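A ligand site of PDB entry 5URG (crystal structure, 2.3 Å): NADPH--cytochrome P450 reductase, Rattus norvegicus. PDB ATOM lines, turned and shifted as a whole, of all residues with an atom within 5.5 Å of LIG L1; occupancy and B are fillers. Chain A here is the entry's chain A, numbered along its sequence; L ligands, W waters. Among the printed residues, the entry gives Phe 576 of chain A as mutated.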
ATOM      1  N   ARG A 242      20.213  -7.714  26.815  1.00  0.00           N
ATOM      2  CA  ARG A 242      20.625  -8.581  25.720  1.00  0.00           C
ATOM      3  C   ARG A 242      22.065  -8.994  25.961  1.00  0.00           C
ATOM      4  O   ARG A 242      22.706  -8.524  26.904  1.00  0.00           O
ATOM      5  CB  ARG A 242      20.530  -7.827  24.392  1.00  0.00           C
ATOM      6  CG  ARG A 242      19.182  -7.170  24.126  1.00  0.00           C
ATOM      7  CD  ARG A 242      19.361  -5.885  23.310  1.00  0.00           C
ATOM      8  NE  ARG A 242      19.832  -6.135  21.956  1.00  0.00           N
ATOM      9  CZ  ARG A 242      20.570  -5.273  21.249  1.00  0.00           C
ATOM     10  NH1 ARG A 242      20.937  -4.104  21.765  1.00  0.00           N
ATOM     11  NH2 ARG A 242      20.931  -5.591  20.020  1.00  0.00           N
ATOM     12  N   LEU A 244      25.616  -9.113  23.956  1.00  0.00           N
ATOM     13  CA  LEU A 244      26.439  -8.848  22.794  1.00  0.00           C
ATOM     14  C   LEU A 244      27.840  -9.318  23.141  1.00  0.00           C
ATOM     15  O   LEU A 244      28.349  -9.035  24.216  1.00  0.00           O
ATOM     16  CB  LEU A 244      26.429  -7.357  22.439  1.00  0.00           C
ATOM     17  CG  LEU A 244      25.124  -7.027  21.717  1.00  0.00           C
ATOM     18  CD1 LEU A 244      24.081  -6.570  22.725  1.00  0.00           C
ATOM     19  CD2 LEU A 244      25.385  -5.943  20.663  1.00  0.00           C
ATOM     20  N   VAL A 418      25.346 -10.228  18.202  1.00  0.00           N
ATOM     21  CA  VAL A 418      24.315 -10.187  19.233  1.00  0.00           C
ATOM     22  C   VAL A 418      23.714 -11.585  19.314  1.00  0.00           C
ATOM     23  O   VAL A 418      23.288 -12.136  18.297  1.00  0.00           O
ATOM     24  CB  VAL A 418      23.177  -9.175  18.905  1.00  0.00           C
ATOM     25  CG1 VAL A 418      22.696  -9.353  17.475  1.00  0.00           C
ATOM     26  CG2 VAL A 418      22.004  -9.407  19.855  1.00  0.00           C
ATOM     27  N   VAL A 420      21.136 -14.422  19.619  1.00  0.00           N
ATOM     28  CA  VAL A 420      19.714 -14.463  19.338  1.00  0.00           C
ATOM     29  C   VAL A 420      19.024 -15.408  20.298  1.00  0.00           C
ATOM     30  O   VAL A 420      19.495 -16.516  20.538  1.00  0.00           O
ATOM     31  CB  VAL A 420      19.450 -14.908  17.891  1.00  0.00           C
ATOM     32  CG1 VAL A 420      17.964 -15.195  17.690  1.00  0.00           C
ATOM     33  CG2 VAL A 420      19.893 -13.812  16.946  1.00  0.00           C
ATOM     34  N   PRO A 477      24.717   1.775  13.312  1.00  0.00           N
ATOM     35  CA  PRO A 477      23.975   1.671  14.581  1.00  0.00           C
ATOM     36  C   PRO A 477      24.033   0.277  15.169  1.00  0.00           C
ATOM     37  O   PRO A 477      24.083  -0.712  14.450  1.00  0.00           O
ATOM     38  CB  PRO A 477      22.561   2.085  14.186  1.00  0.00           C
ATOM     39  CG  PRO A 477      22.480   1.692  12.733  1.00  0.00           C
ATOM     40  CD  PRO A 477      23.813   2.106  12.194  1.00  0.00           C
ATOM     41  N   GLY A 478      24.029   0.209  16.498  1.00  0.00           N
ATOM     42  CA  GLY A 478      24.060  -1.073  17.175  1.00  0.00           C
ATOM     43  C   GLY A 478      25.198  -1.973  16.736  1.00  0.00           C
ATOM     44  O   GLY A 478      26.335  -1.532  16.605  1.00  0.00           O
ATOM     45  N   THR A 479      24.872  -3.229  16.479  1.00  0.00           N
ATOM     46  CA  THR A 479      25.854  -4.213  16.059  1.00  0.00           C
ATOM     47  C   THR A 479      26.543  -3.844  14.745  1.00  0.00           C
ATOM     48  O   THR A 479      27.586  -4.393  14.426  1.00  0.00           O
ATOM     49  CB  THR A 479      25.195  -5.577  15.916  1.00  0.00           C
ATOM     50  OG1 THR A 479      24.415  -5.835  17.082  1.00  0.00           O
ATOM     51  CG2 THR A 479      26.236  -6.659  15.765  1.00  0.00           C
ATOM     52  N   GLY A 480      25.943  -2.924  14.001  1.00  0.00           N
ATOM     53  CA  GLY A 480      26.523  -2.495  12.747  1.00  0.00           C
ATOM     54  C   GLY A 480      27.891  -1.855  12.956  1.00  0.00           C
ATOM     55  O   GLY A 480      28.579  -1.496  12.012  1.00  0.00           O
ATOM     56  N   GLY A 509      25.340   4.266  17.241  1.00  0.00           N
ATOM     57  CA  GLY A 509      24.116   4.404  18.012  1.00  0.00           C
ATOM     58  C   GLY A 509      23.830   3.192  18.887  1.00  0.00           C
ATOM     59  O   GLY A 509      24.156   2.061  18.522  1.00  0.00           O
ATOM     60  N   CYS A 510      23.244   3.427  20.048  1.00  0.00           N
ATOM     61  CA  CYS A 510      22.887   2.348  20.959  1.00  0.00           C
ATOM     62  C   CYS A 510      21.730   2.841  21.818  1.00  0.00           C
ATOM     63  O   CYS A 510      21.298   3.988  21.680  1.00  0.00           O
ATOM     64  CB  CYS A 510      24.073   1.937  21.840  1.00  0.00           C
ATOM     65  SG  CYS A 510      24.704   3.196  22.933  1.00  0.00           S
ATOM     66  N   ARG A 511      21.220   1.983  22.687  1.00  0.00           N
ATOM     67  CA  ARG A 511      20.071   2.361  23.512  1.00  0.00           C
ATOM     68  C   ARG A 511      20.396   3.265  24.708  1.00  0.00           C
ATOM     69  O   ARG A 511      19.658   4.219  24.969  1.00  0.00           O
ATOM     70  CB  ARG A 511      19.341   1.101  23.984  1.00  0.00           C
ATOM     71  CG  ARG A 511      19.036   0.137  22.843  1.00  0.00           C
ATOM     72  CD  ARG A 511      18.333  -1.134  23.316  1.00  0.00           C
ATOM     73  NE  ARG A 511      18.031  -2.019  22.196  1.00  0.00           N
ATOM     74  CZ  ARG A 511      17.298  -3.127  22.290  1.00  0.00           C
ATOM     75  NH1 ARG A 511      16.795  -3.524  23.454  1.00  0.00           N
ATOM     76  NH2 ARG A 511      17.058  -3.842  21.201  1.00  0.00           N
ATOM     77  N   ASP A 516      24.191  -0.858  26.366  1.00  0.00           N
ATOM     78  CA  ASP A 516      24.823  -1.514  25.226  1.00  0.00           C
ATOM     79  C   ASP A 516      25.689  -0.637  24.306  1.00  0.00           C
ATOM     80  O   ASP A 516      25.571  -0.708  23.079  1.00  0.00           O
ATOM     81  CB  ASP A 516      23.750  -2.206  24.390  1.00  0.00           C
ATOM     82  CG  ASP A 516      22.649  -1.252  23.931  1.00  0.00           C
ATOM     83  OD1 ASP A 516      22.789  -0.019  24.120  1.00  0.00           O
ATOM     84  OD2 ASP A 516      21.645  -1.735  23.376  1.00  0.00           O
ATOM     85  N   ALA A 538      24.424   8.217  19.069  1.00  0.00           N
ATOM     86  CA  ALA A 538      23.019   8.481  19.295  1.00  0.00           C
ATOM     87  C   ALA A 538      22.565   7.503  20.380  1.00  0.00           C
ATOM     88  O   ALA A 538      22.664   6.293  20.201  1.00  0.00           O
ATOM     89  CB  ALA A 538      22.216   8.252  18.003  1.00  0.00           C
ATOM     90  N   SER A 540      19.557   6.285  21.720  1.00  0.00           N
ATOM     91  CA  SER A 540      18.137   6.237  21.411  1.00  0.00           C
ATOM     92  C   SER A 540      17.169   6.257  22.583  1.00  0.00           C
ATOM     93  O   SER A 540      16.038   6.719  22.439  1.00  0.00           O
ATOM     94  CB  SER A 540      17.826   5.020  20.525  1.00  0.00           C
ATOM     95  OG  SER A 540      18.143   3.803  21.161  1.00  0.00           O
ATOM     96  N   ARG A 541      17.605   5.787  23.742  1.00  0.00           N
ATOM     97  CA  ARG A 541      16.684   5.757  24.869  1.00  0.00           C
ATOM     98  C   ARG A 541      17.066   6.532  26.121  1.00  0.00           C
ATOM     99  O   ARG A 541      16.558   6.234  27.195  1.00  0.00           O
ATOM    100  CB  ARG A 541      16.408   4.294  25.259  1.00  0.00           C
ATOM    101  CG  ARG A 541      16.098   3.423  24.041  1.00  0.00           C
ATOM    102  CD  ARG A 541      15.658   2.012  24.407  1.00  0.00           C
ATOM    103  NE  ARG A 541      15.370   1.252  23.195  1.00  0.00           N
ATOM    104  CZ  ARG A 541      14.927   0.001  23.171  1.00  0.00           C
ATOM    105  NH1 ARG A 541      14.704  -0.638  24.308  1.00  0.00           N
ATOM    106  NH2 ARG A 541      14.714  -0.612  22.018  1.00  0.00           N
ATOM    107  N   LYS A 546      13.138   9.492  20.380  1.00  0.00           N
ATOM    108  CA  LYS A 546      14.185   8.654  19.815  1.00  0.00           C
ATOM    109  C   LYS A 546      15.254   9.556  19.199  1.00  0.00           C
ATOM    110  O   LYS A 546      14.947  10.579  18.598  1.00  0.00           O
ATOM    111  CB  LYS A 546      13.618   7.757  18.708  1.00  0.00           C
ATOM    112  CG  LYS A 546      12.669   6.650  19.172  1.00  0.00           C
ATOM    113  CD  LYS A 546      13.329   5.718  20.194  1.00  0.00           C
ATOM    114  CE  LYS A 546      12.464   4.489  20.441  1.00  0.00           C
ATOM    115  NZ  LYS A 546      13.037   3.612  21.504  1.00  0.00           N
ATOM    116  N   TYR A 548      18.498   8.918  16.739  1.00  0.00           N
ATOM    117  CA  TYR A 548      19.233   7.943  15.937  1.00  0.00           C
ATOM    118  C   TYR A 548      20.415   8.577  15.208  1.00  0.00           C
ATOM    119  O   TYR A 548      20.560   9.791  15.166  1.00  0.00           O
ATOM    120  CB  TYR A 548      18.300   7.300  14.907  1.00  0.00           C
ATOM    121  CG  TYR A 548      17.106   6.566  15.490  1.00  0.00           C
ATOM    122  CD1 TYR A 548      17.244   5.754  16.628  1.00  0.00           C
ATOM    123  CD2 TYR A 548      15.859   6.625  14.872  1.00  0.00           C
ATOM    124  CE1 TYR A 548      16.171   5.016  17.133  1.00  0.00           C
ATOM    125  CE2 TYR A 548      14.771   5.874  15.362  1.00  0.00           C
ATOM    126  CZ  TYR A 548      14.939   5.072  16.490  1.00  0.00           C
ATOM    127  OH  TYR A 548      13.895   4.293  16.939  1.00  0.00           O
ATOM    128  N   VAL A 549      21.256   7.740  14.621  1.00  0.00           N
ATOM    129  CA  VAL A 549      22.403   8.250  13.895  1.00  0.00           C
ATOM    130  C   VAL A 549      22.055   9.301  12.831  1.00  0.00           C
ATOM    131  O   VAL A 549      22.821  10.245  12.651  1.00  0.00           O
ATOM    132  CB  VAL A 549      23.203   7.103  13.230  1.00  0.00           C
ATOM    133  CG1 VAL A 549      23.954   6.322  14.297  1.00  0.00           C
ATOM    134  CG2 VAL A 549      22.261   6.200  12.443  1.00  0.00           C
ATOM    135  N   GLN A 550      20.926   9.170  12.144  1.00  0.00           N
ATOM    136  CA  GLN A 550      20.602  10.139  11.090  1.00  0.00           C
ATOM    137  C   GLN A 550      20.301  11.526  11.633  1.00  0.00           C
ATOM    138  O   GLN A 550      20.485  12.520  10.952  1.00  0.00           O
ATOM    139  CB  GLN A 550      19.429   9.669  10.219  1.00  0.00           C
ATOM    140  CG  GLN A 550      18.163   9.370  10.977  1.00  0.00           C
ATOM    141  CD  GLN A 550      18.094   7.928  11.417  1.00  0.00           C
ATOM    142  OE1 GLN A 550      19.104   7.351  11.823  1.00  0.00           O
ATOM    143  NE2 GLN A 550      16.902   7.349  11.355  1.00  0.00           N
ATOM    144  N   PHE A 576      21.656  -4.124  10.719  1.00  0.00           N
ATOM    145  CA  PHE A 576      20.596  -5.068  10.398  1.00  0.00           C
ATOM    146  C   PHE A 576      19.444  -4.446   9.604  1.00  0.00           C
ATOM    147  O   PHE A 576      19.161  -4.877   8.491  1.00  0.00           O
ATOM    148  CB  PHE A 576      20.007  -5.659  11.681  1.00  0.00           C
ATOM    149  CG  PHE A 576      20.801  -6.810  12.235  1.00  0.00           C
ATOM    150  CD1 PHE A 576      20.783  -8.044  11.612  1.00  0.00           C
ATOM    151  CD2 PHE A 576      21.605  -6.626  13.363  1.00  0.00           C
ATOM    152  CE1 PHE A 576      21.556  -9.093  12.102  1.00  0.00           C
ATOM    153  CE2 PHE A 576      22.374  -7.667  13.857  1.00  0.00           C
ATOM    154  CZ  PHE A 576      22.363  -8.903  13.242  1.00  0.00           C
ATOM    155  N   ALA A 577      18.796  -3.452  10.189  1.00  0.00           N
ATOM    156  CA  ALA A 577      17.628  -2.797   9.609  1.00  0.00           C
ATOM    157  C   ALA A 577      17.745  -2.138   8.249  1.00  0.00           C
ATOM    158  O   ALA A 577      18.469  -1.152   8.069  1.00  0.00           O
ATOM    159  CB  ALA A 577      17.042  -1.813  10.602  1.00  0.00           C
ATOM    160  N   ASN A 579      15.370  -0.603   6.951  1.00  0.00           N
ATOM    161  CA  ASN A 579      14.686   0.677   7.097  1.00  0.00           C
ATOM    162  C   ASN A 579      15.670   1.734   7.613  1.00  0.00           C
ATOM    163  O   ASN A 579      15.596   2.897   7.212  1.00  0.00           O
ATOM    164  CB  ASN A 579      13.482   0.564   8.033  1.00  0.00           C
ATOM    165  CG  ASN A 579      13.767  -0.276   9.268  1.00  0.00           C
ATOM    166  OD1 ASN A 579      14.073  -1.480   9.164  1.00  0.00           O
ATOM    167  ND2 ASN A 579      13.667   0.340  10.452  1.00  0.00           N
ATOM    168  N   MET A 580      16.581   1.328   8.493  1.00  0.00           N
ATOM    169  CA  MET A 580      17.586   2.232   9.028  1.00  0.00           C
ATOM    170  C   MET A 580      18.431   2.730   7.860  1.00  0.00           C
ATOM    171  O   MET A 580      18.722   3.916   7.742  1.00  0.00           O
ATOM    172  CB  MET A 580      18.446   1.492  10.060  1.00  0.00           C
ATOM    173  CG  MET A 580      19.663   2.251  10.582  1.00  0.00           C
ATOM    174  SD  MET A 580      21.050   2.292   9.414  1.00  0.00           S
ATOM    175  CE  MET A 580      21.650   0.642   9.564  1.00  0.00           C
ATOM    176  N   ASP A 583      16.418   5.256   5.965  1.00  0.00           N
ATOM    177  CA  ASP A 583      16.322   6.522   6.690  1.00  0.00           C
ATOM    178  C   ASP A 583      17.622   7.296   6.536  1.00  0.00           C
ATOM    179  O   ASP A 583      17.620   8.501   6.262  1.00  0.00           O
ATOM    180  CB  ASP A 583      16.033   6.284   8.178  1.00  0.00           C
ATOM    181  CG  ASP A 583      14.634   5.739   8.415  1.00  0.00           C
ATOM    182  OD1 ASP A 583      13.763   5.933   7.544  1.00  0.00           O
ATOM    183  OD2 ASP A 583      14.416   5.142   9.486  1.00  0.00           O
HETATM  184  P1  LIG L   1      19.416  -2.427  18.419  1.00  0.00           P
HETATM  185  O1  LIG L   1      19.582  -1.982  19.819  1.00  0.00           O
HETATM  186  O2  LIG L   1      18.052  -2.665  17.895  1.00  0.00           O
HETATM  187  O3  LIG L   1      20.216  -1.412  17.465  1.00  0.00           O
HETATM  188  C1  LIG L   1      19.552  -0.382  16.735  1.00  0.00           C
HETATM  189  C2  LIG L   1      20.004   0.961  17.316  1.00  0.00           C
HETATM  190  O4  LIG L   1      19.604   2.000  16.400  1.00  0.00           O
HETATM  191  C3  LIG L   1      19.220   1.255  18.585  1.00  0.00           C
HETATM  192  O5  LIG L   1      19.797   2.367  19.285  1.00  0.00           O
HETATM  193  C4  LIG L   1      17.869   1.593  17.982  1.00  0.00           C
HETATM  194  O6  LIG L   1      17.136   2.433  18.887  1.00  0.00           O
HETATM  195  C5  LIG L   1      18.300   2.437  16.797  1.00  0.00           C
HETATM  196  N1  LIG L   1      17.347   2.404  15.667  1.00  0.00           N
HETATM  197  C6  LIG L   1      16.206   1.703  15.601  1.00  0.00           C
HETATM  198  N2  LIG L   1      15.605   2.033  14.461  1.00  0.00           N
HETATM  199  C7  LIG L   1      16.354   2.924  13.828  1.00  0.00           C
HETATM  200  C8  LIG L   1      16.191   3.547  12.663  1.00  0.00           C
HETATM  201  N3  LIG L   1      15.033   3.342  12.033  1.00  0.00           N
HETATM  202  N4  LIG L   1      17.118   4.370  12.160  1.00  0.00           N
HETATM  203  C9  LIG L   1      18.294   4.588  12.895  1.00  0.00           C
HETATM  204  N5  LIG L   1      18.419   3.943  14.129  1.00  0.00           N
HETATM  205  C10 LIG L   1      17.440   3.133  14.560  1.00  0.00           C
HETATM  206  O7  LIG L   1      20.289  -3.764  18.198  1.00  0.00           O
HETATM  207  P2  LIG L   1      20.977  -4.289  16.839  1.00  0.00           P
HETATM  208  O8  LIG L   1      21.708  -5.541  17.132  1.00  0.00           O
HETATM  209  O9  LIG L   1      21.718  -3.175  16.210  1.00  0.00           O
HETATM  210  O10 LIG L   1      19.696  -4.622  15.916  1.00  0.00           O
HETATM  211  C11 LIG L   1      18.990  -3.549  15.293  1.00  0.00           C
HETATM  212  C12 LIG L   1      17.697  -4.049  14.626  1.00  0.00           C
HETATM  213  O11 LIG L   1      17.934  -5.075  13.663  1.00  0.00           O
HETATM  214  C13 LIG L   1      16.738  -4.654  15.629  1.00  0.00           C
HETATM  215  O12 LIG L   1      16.030  -3.628  16.322  1.00  0.00           O
HETATM  216  C14 LIG L   1      15.796  -5.309  14.632  1.00  0.00           C
HETATM  217  O13 LIG L   1      15.084  -4.309  13.886  1.00  0.00           O
HETATM  218  C15 LIG L   1      16.811  -5.976  13.717  1.00  0.00           C
HETATM  219  N6  LIG L   1      17.282  -7.259  14.281  1.00  0.00           N
HETATM  220  C16 LIG L   1      16.645  -8.450  13.928  1.00  0.00           C
HETATM  221  C17 LIG L   1      17.224  -9.673  14.248  1.00  0.00           C
HETATM  222  C18 LIG L   1      18.400  -9.705  14.995  1.00  0.00           C
HETATM  223  C19 LIG L   1      19.022  -8.519  15.387  1.00  0.00           C
HETATM  224  C20 LIG L   1      18.475  -7.294  15.027  1.00  0.00           C
HETATM  225  P3  LIG L   1      15.725   1.982  19.528  1.00  0.00           P
HETATM  226  O14 LIG L   1      14.734   2.405  18.521  1.00  0.00           O
HETATM  227  O15 LIG L   1      15.685   2.747  20.796  1.00  0.00           O
HETATM  228  O16 LIG L   1      15.857   0.521  19.702  1.00  0.00           O
HETATM  229  P1  LG2 L   2      19.432 -18.308  13.410  1.00  0.00           P
HETATM  230  O1  LG2 L   2      19.191 -19.652  13.981  1.00  0.00           O
HETATM  231  O2  LG2 L   2      20.031 -18.212  12.064  1.00  0.00           O
HETATM  232  O3  LG2 L   2      18.047 -17.499  13.442  1.00  0.00           O
HETATM  233  C1  LG2 L   2      17.912 -16.267  12.731  1.00  0.00           C
HETATM  234  C2  LG2 L   2      16.426 -16.019  12.444  1.00  0.00           C
HETATM  235  O4  LG2 L   2      15.665 -16.008  13.650  1.00  0.00           O
HETATM  236  C3  LG2 L   2      16.199 -14.629  11.881  1.00  0.00           C
HETATM  237  O5  LG2 L   2      16.521 -14.630  10.484  1.00  0.00           O
HETATM  238  C4  LG2 L   2      14.682 -14.593  12.020  1.00  0.00           C
HETATM  239  O6  LG2 L   2      14.083 -15.349  10.970  1.00  0.00           O
HETATM  240  C5  LG2 L   2      14.467 -15.273  13.369  1.00  0.00           C
HETATM  241  N1  LG2 L   2      14.349 -14.284  14.464  1.00  0.00           N
HETATM  242  C6  LG2 L   2      15.470 -13.588  15.115  1.00  0.00           C
HETATM  243  N2  LG2 L   2      14.758 -12.870  16.186  1.00  0.00           N
HETATM  244  C7  LG2 L   2      13.445 -13.053  16.034  1.00  0.00           C
HETATM  245  C8  LG2 L   2      12.446 -12.592  16.767  1.00  0.00           C
HETATM  246  N3  LG2 L   2      12.784 -11.940  17.883  1.00  0.00           N
HETATM  247  N4  LG2 L   2      11.164 -12.895  16.521  1.00  0.00           N
HETATM  248  C9  LG2 L   2      10.866 -13.738  15.442  1.00  0.00           C
HETATM  249  N5  LG2 L   2      11.954 -14.212  14.684  1.00  0.00           N
HETATM  250  C10 LG2 L   2      13.208 -13.862  14.998  1.00  0.00           C
HETATM  251  N6  LG2 L   2      25.090 -10.538  12.948  1.00  0.00           N
HETATM  252  C11 LG2 L   2      25.855 -10.007  13.990  1.00  0.00           C
HETATM  253  O7  LG2 L   2      25.407  -9.984  15.140  1.00  0.00           O
HETATM  254  N7  LG2 L   2      27.102  -9.427  13.701  1.00  0.00           N
HETATM  255  C12 LG2 L   2      27.571  -9.391  12.380  1.00  0.00           C
HETATM  256  O8  LG2 L   2      28.718  -9.024  12.167  1.00  0.00           O
HETATM  257  C13 LG2 L   2      26.772  -9.881  11.346  1.00  0.00           C
HETATM  258  N8  LG2 L   2      27.093  -9.608  10.072  1.00  0.00           N
HETATM  259  C14 LG2 L   2      26.332 -10.104   9.083  1.00  0.00           C
HETATM  260  C15 LG2 L   2      26.754  -9.954   7.763  1.00  0.00           C
HETATM  261  C16 LG2 L   2      26.068 -10.590   6.733  1.00  0.00           C
HETATM  262  C17 LG2 L   2      26.570 -10.551   5.438  1.00  0.00           C
HETATM  263  C18 LG2 L   2      24.947 -11.359   7.026  1.00  0.00           C
HETATM  264  C19 LG2 L   2      24.292 -12.035   6.006  1.00  0.00           C
HETATM  265  C20 LG2 L   2      24.527 -11.495   8.346  1.00  0.00           C
HETATM  266  C21 LG2 L   2      25.225 -10.890   9.374  1.00  0.00           C
HETATM  267  N9  LG2 L   2      24.905 -11.134  10.664  1.00  0.00           N
HETATM  268  C22 LG2 L   2      25.538 -10.449  11.625  1.00  0.00           C
HETATM  269  C23 LG2 L   2      23.748 -11.984  11.017  1.00  0.00           C
HETATM  270  C24 LG2 L   2      24.224 -13.438  11.109  1.00  0.00           C
HETATM  271  O9  LG2 L   2      24.656 -13.881   9.832  1.00  0.00           O
HETATM  272  C25 LG2 L   2      23.129 -14.373  11.624  1.00  0.00           C
HETATM  273  O10 LG2 L   2      21.961 -14.285  10.811  1.00  0.00           O
HETATM  274  C26 LG2 L   2      22.786 -14.032  13.077  1.00  0.00           C
HETATM  275  O11 LG2 L   2      23.981 -14.081  13.872  1.00  0.00           O
HETATM  276  C27 LG2 L   2      21.775 -15.044  13.605  1.00  0.00           C
HETATM  277  O12 LG2 L   2      22.266 -16.369  13.355  1.00  0.00           O
HETATM  278  P2  LG2 L   2      21.958 -17.583  14.368  1.00  0.00           P
HETATM  279  O13 LG2 L   2      22.236 -18.868  13.671  1.00  0.00           O
HETATM  280  O14 LG2 L   2      22.445 -17.335  15.748  1.00  0.00           O
HETATM  281  O15 LG2 L   2      20.361 -17.486  14.436  1.00  0.00           O
HETATM  282  O   HOH W   1      21.754  -0.826  20.889  1.00  0.00           O
HETATM  283  O   HOH W   2      20.725 -11.200  15.047  1.00  0.00           O
HETATM  284  O   HOH W   3      12.364   1.281  13.913  1.00  0.00           O
HETATM  285  O   HOH W   4      20.737   4.832  15.468  1.00  0.00           O
HETATM  286  O   HOH W   5      18.298   0.133  13.243  1.00  0.00           O
HETATM  287  O   HOH W   6      20.677   4.821  18.370  1.00  0.00           O
HETATM  288  O   HOH W   7      22.368  -2.646  13.588  1.00  0.00           O
HETATM  289  O   HOH W   8      23.681  -3.836  19.186  1.00  0.00           O
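The side-chain hydroxyl of Tyr 548 sits at hydrogen-bond distance from an oxygen (O14) of LIG L1 (2.6 Å).
O8 of LIG L1 is in salt-bridge range of NH2 of Arg 242, 3.0 Å away.
O15 of LIG L1 sits at hydrogen-bond distance from OG of Ser 540.
The backbone NH of Thr 479 sits at hydrogen-bond distance from an oxygen (O9) of LIG L1 (3.2 Å).
The side-chain hydroxyl (OG1) of Thr 479 is in hydrogen-bond range of an oxygen (O8) of LIG L1, 2.7 Å away.
The guanidinium group (NH2) of Arg 541 is in salt-bridge range of an oxygen (O16) of LIG L1 (2.8 Å).
An oxygen (O1) of LIG L1 is in salt-bridge range of the guanidinium group (NE) of Arg 511, 2.8 Å away.
An oxygen (O15) of LIG L1 lies within salt-bridge range of the side-chain amino group of Lys 546 (2.9 Å).
N4 of LIG L1 lies within hydrogen-bond range of NE2 of Gln 550 (3.1 Å).
N3 of LIG L1 lies within hydrogen-bond range of OD2 of Asp 583, at 3.2 Å.
The backbone carbonyl oxygen of Cys 510 lies close to an oxygen (O5) of LIG L1, at 3.3 Å.
The backbone NH of Val 418 lies within hydrogen-bond range of an oxygen (O7) of LG2 L2.
OD2 of Asp 516 lies within salt-bridge range of NH1 of Arg 242 (3.0 Å).
The backbone carbonyl oxygen of Cys 510 lies within hydrogen-bond range of the backbone NH of Ser 540.
The backbone NH (N) of Arg 541 lies within hydrogen-bond range of the backbone carbonyl oxygen (O) of Arg 511 (2.9 Å).
NE of Arg 511 lies within salt-bridge range of OD2 of Asp 516 (3.8 Å).
N of Cys 510 lies within hydrogen-bond range of O of Ala 538.
O of Gly 509 sits at hydrogen-bond distance from N of Gly 478, 2.7 Å away.
Residues that only touch LIG L1: Phe 576 (2.9 Å), Gly 478 (3.3 Å), Met 580 (3.6 Å), Asn 579 (3.7 Å), Pro 477 (3.7 Å), Ala 577 (3.9 Å) and Val 418 (3.95 Å).
Hydrophobic or aromatic side chains that line LIG L1: Val 418, Pro 477, Tyr 548, Phe 576 and Met 580.
The nearest printed residue that does not touch LIG L1 is Asp 516 (4.1 Å).
Water W1 lies within hydrogen-bond range of OD2 of Asp 516 (2.7 Å), O1 of LIG L1 (2.7 Å), N of Arg 511 (3.4 Å) and NH1 of Arg 242 (3.5 Å).
Water W7 lies within hydrogen-bond range of O of Pro 477, O9 of LIG L1 and N of Phe 576.
Water W6 lies within hydrogen-bond range of an oxygen (O5) of LIG L1, the backbone carbonyl oxygen (O) of Ala 538 and the backbone NH (N) of Cys 510.
Water W4 bridges a nitrogen (N5) of LIG L1 and the backbone NH of Val 549.
Water W8 lies within hydrogen-bond range of the side-chain hydroxyl of Thr 479 (3.0 Å), an oxygen (O8) of LIG L1 (3.3 Å) and the guanidinium group of Arg 242 (3.4 Å).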
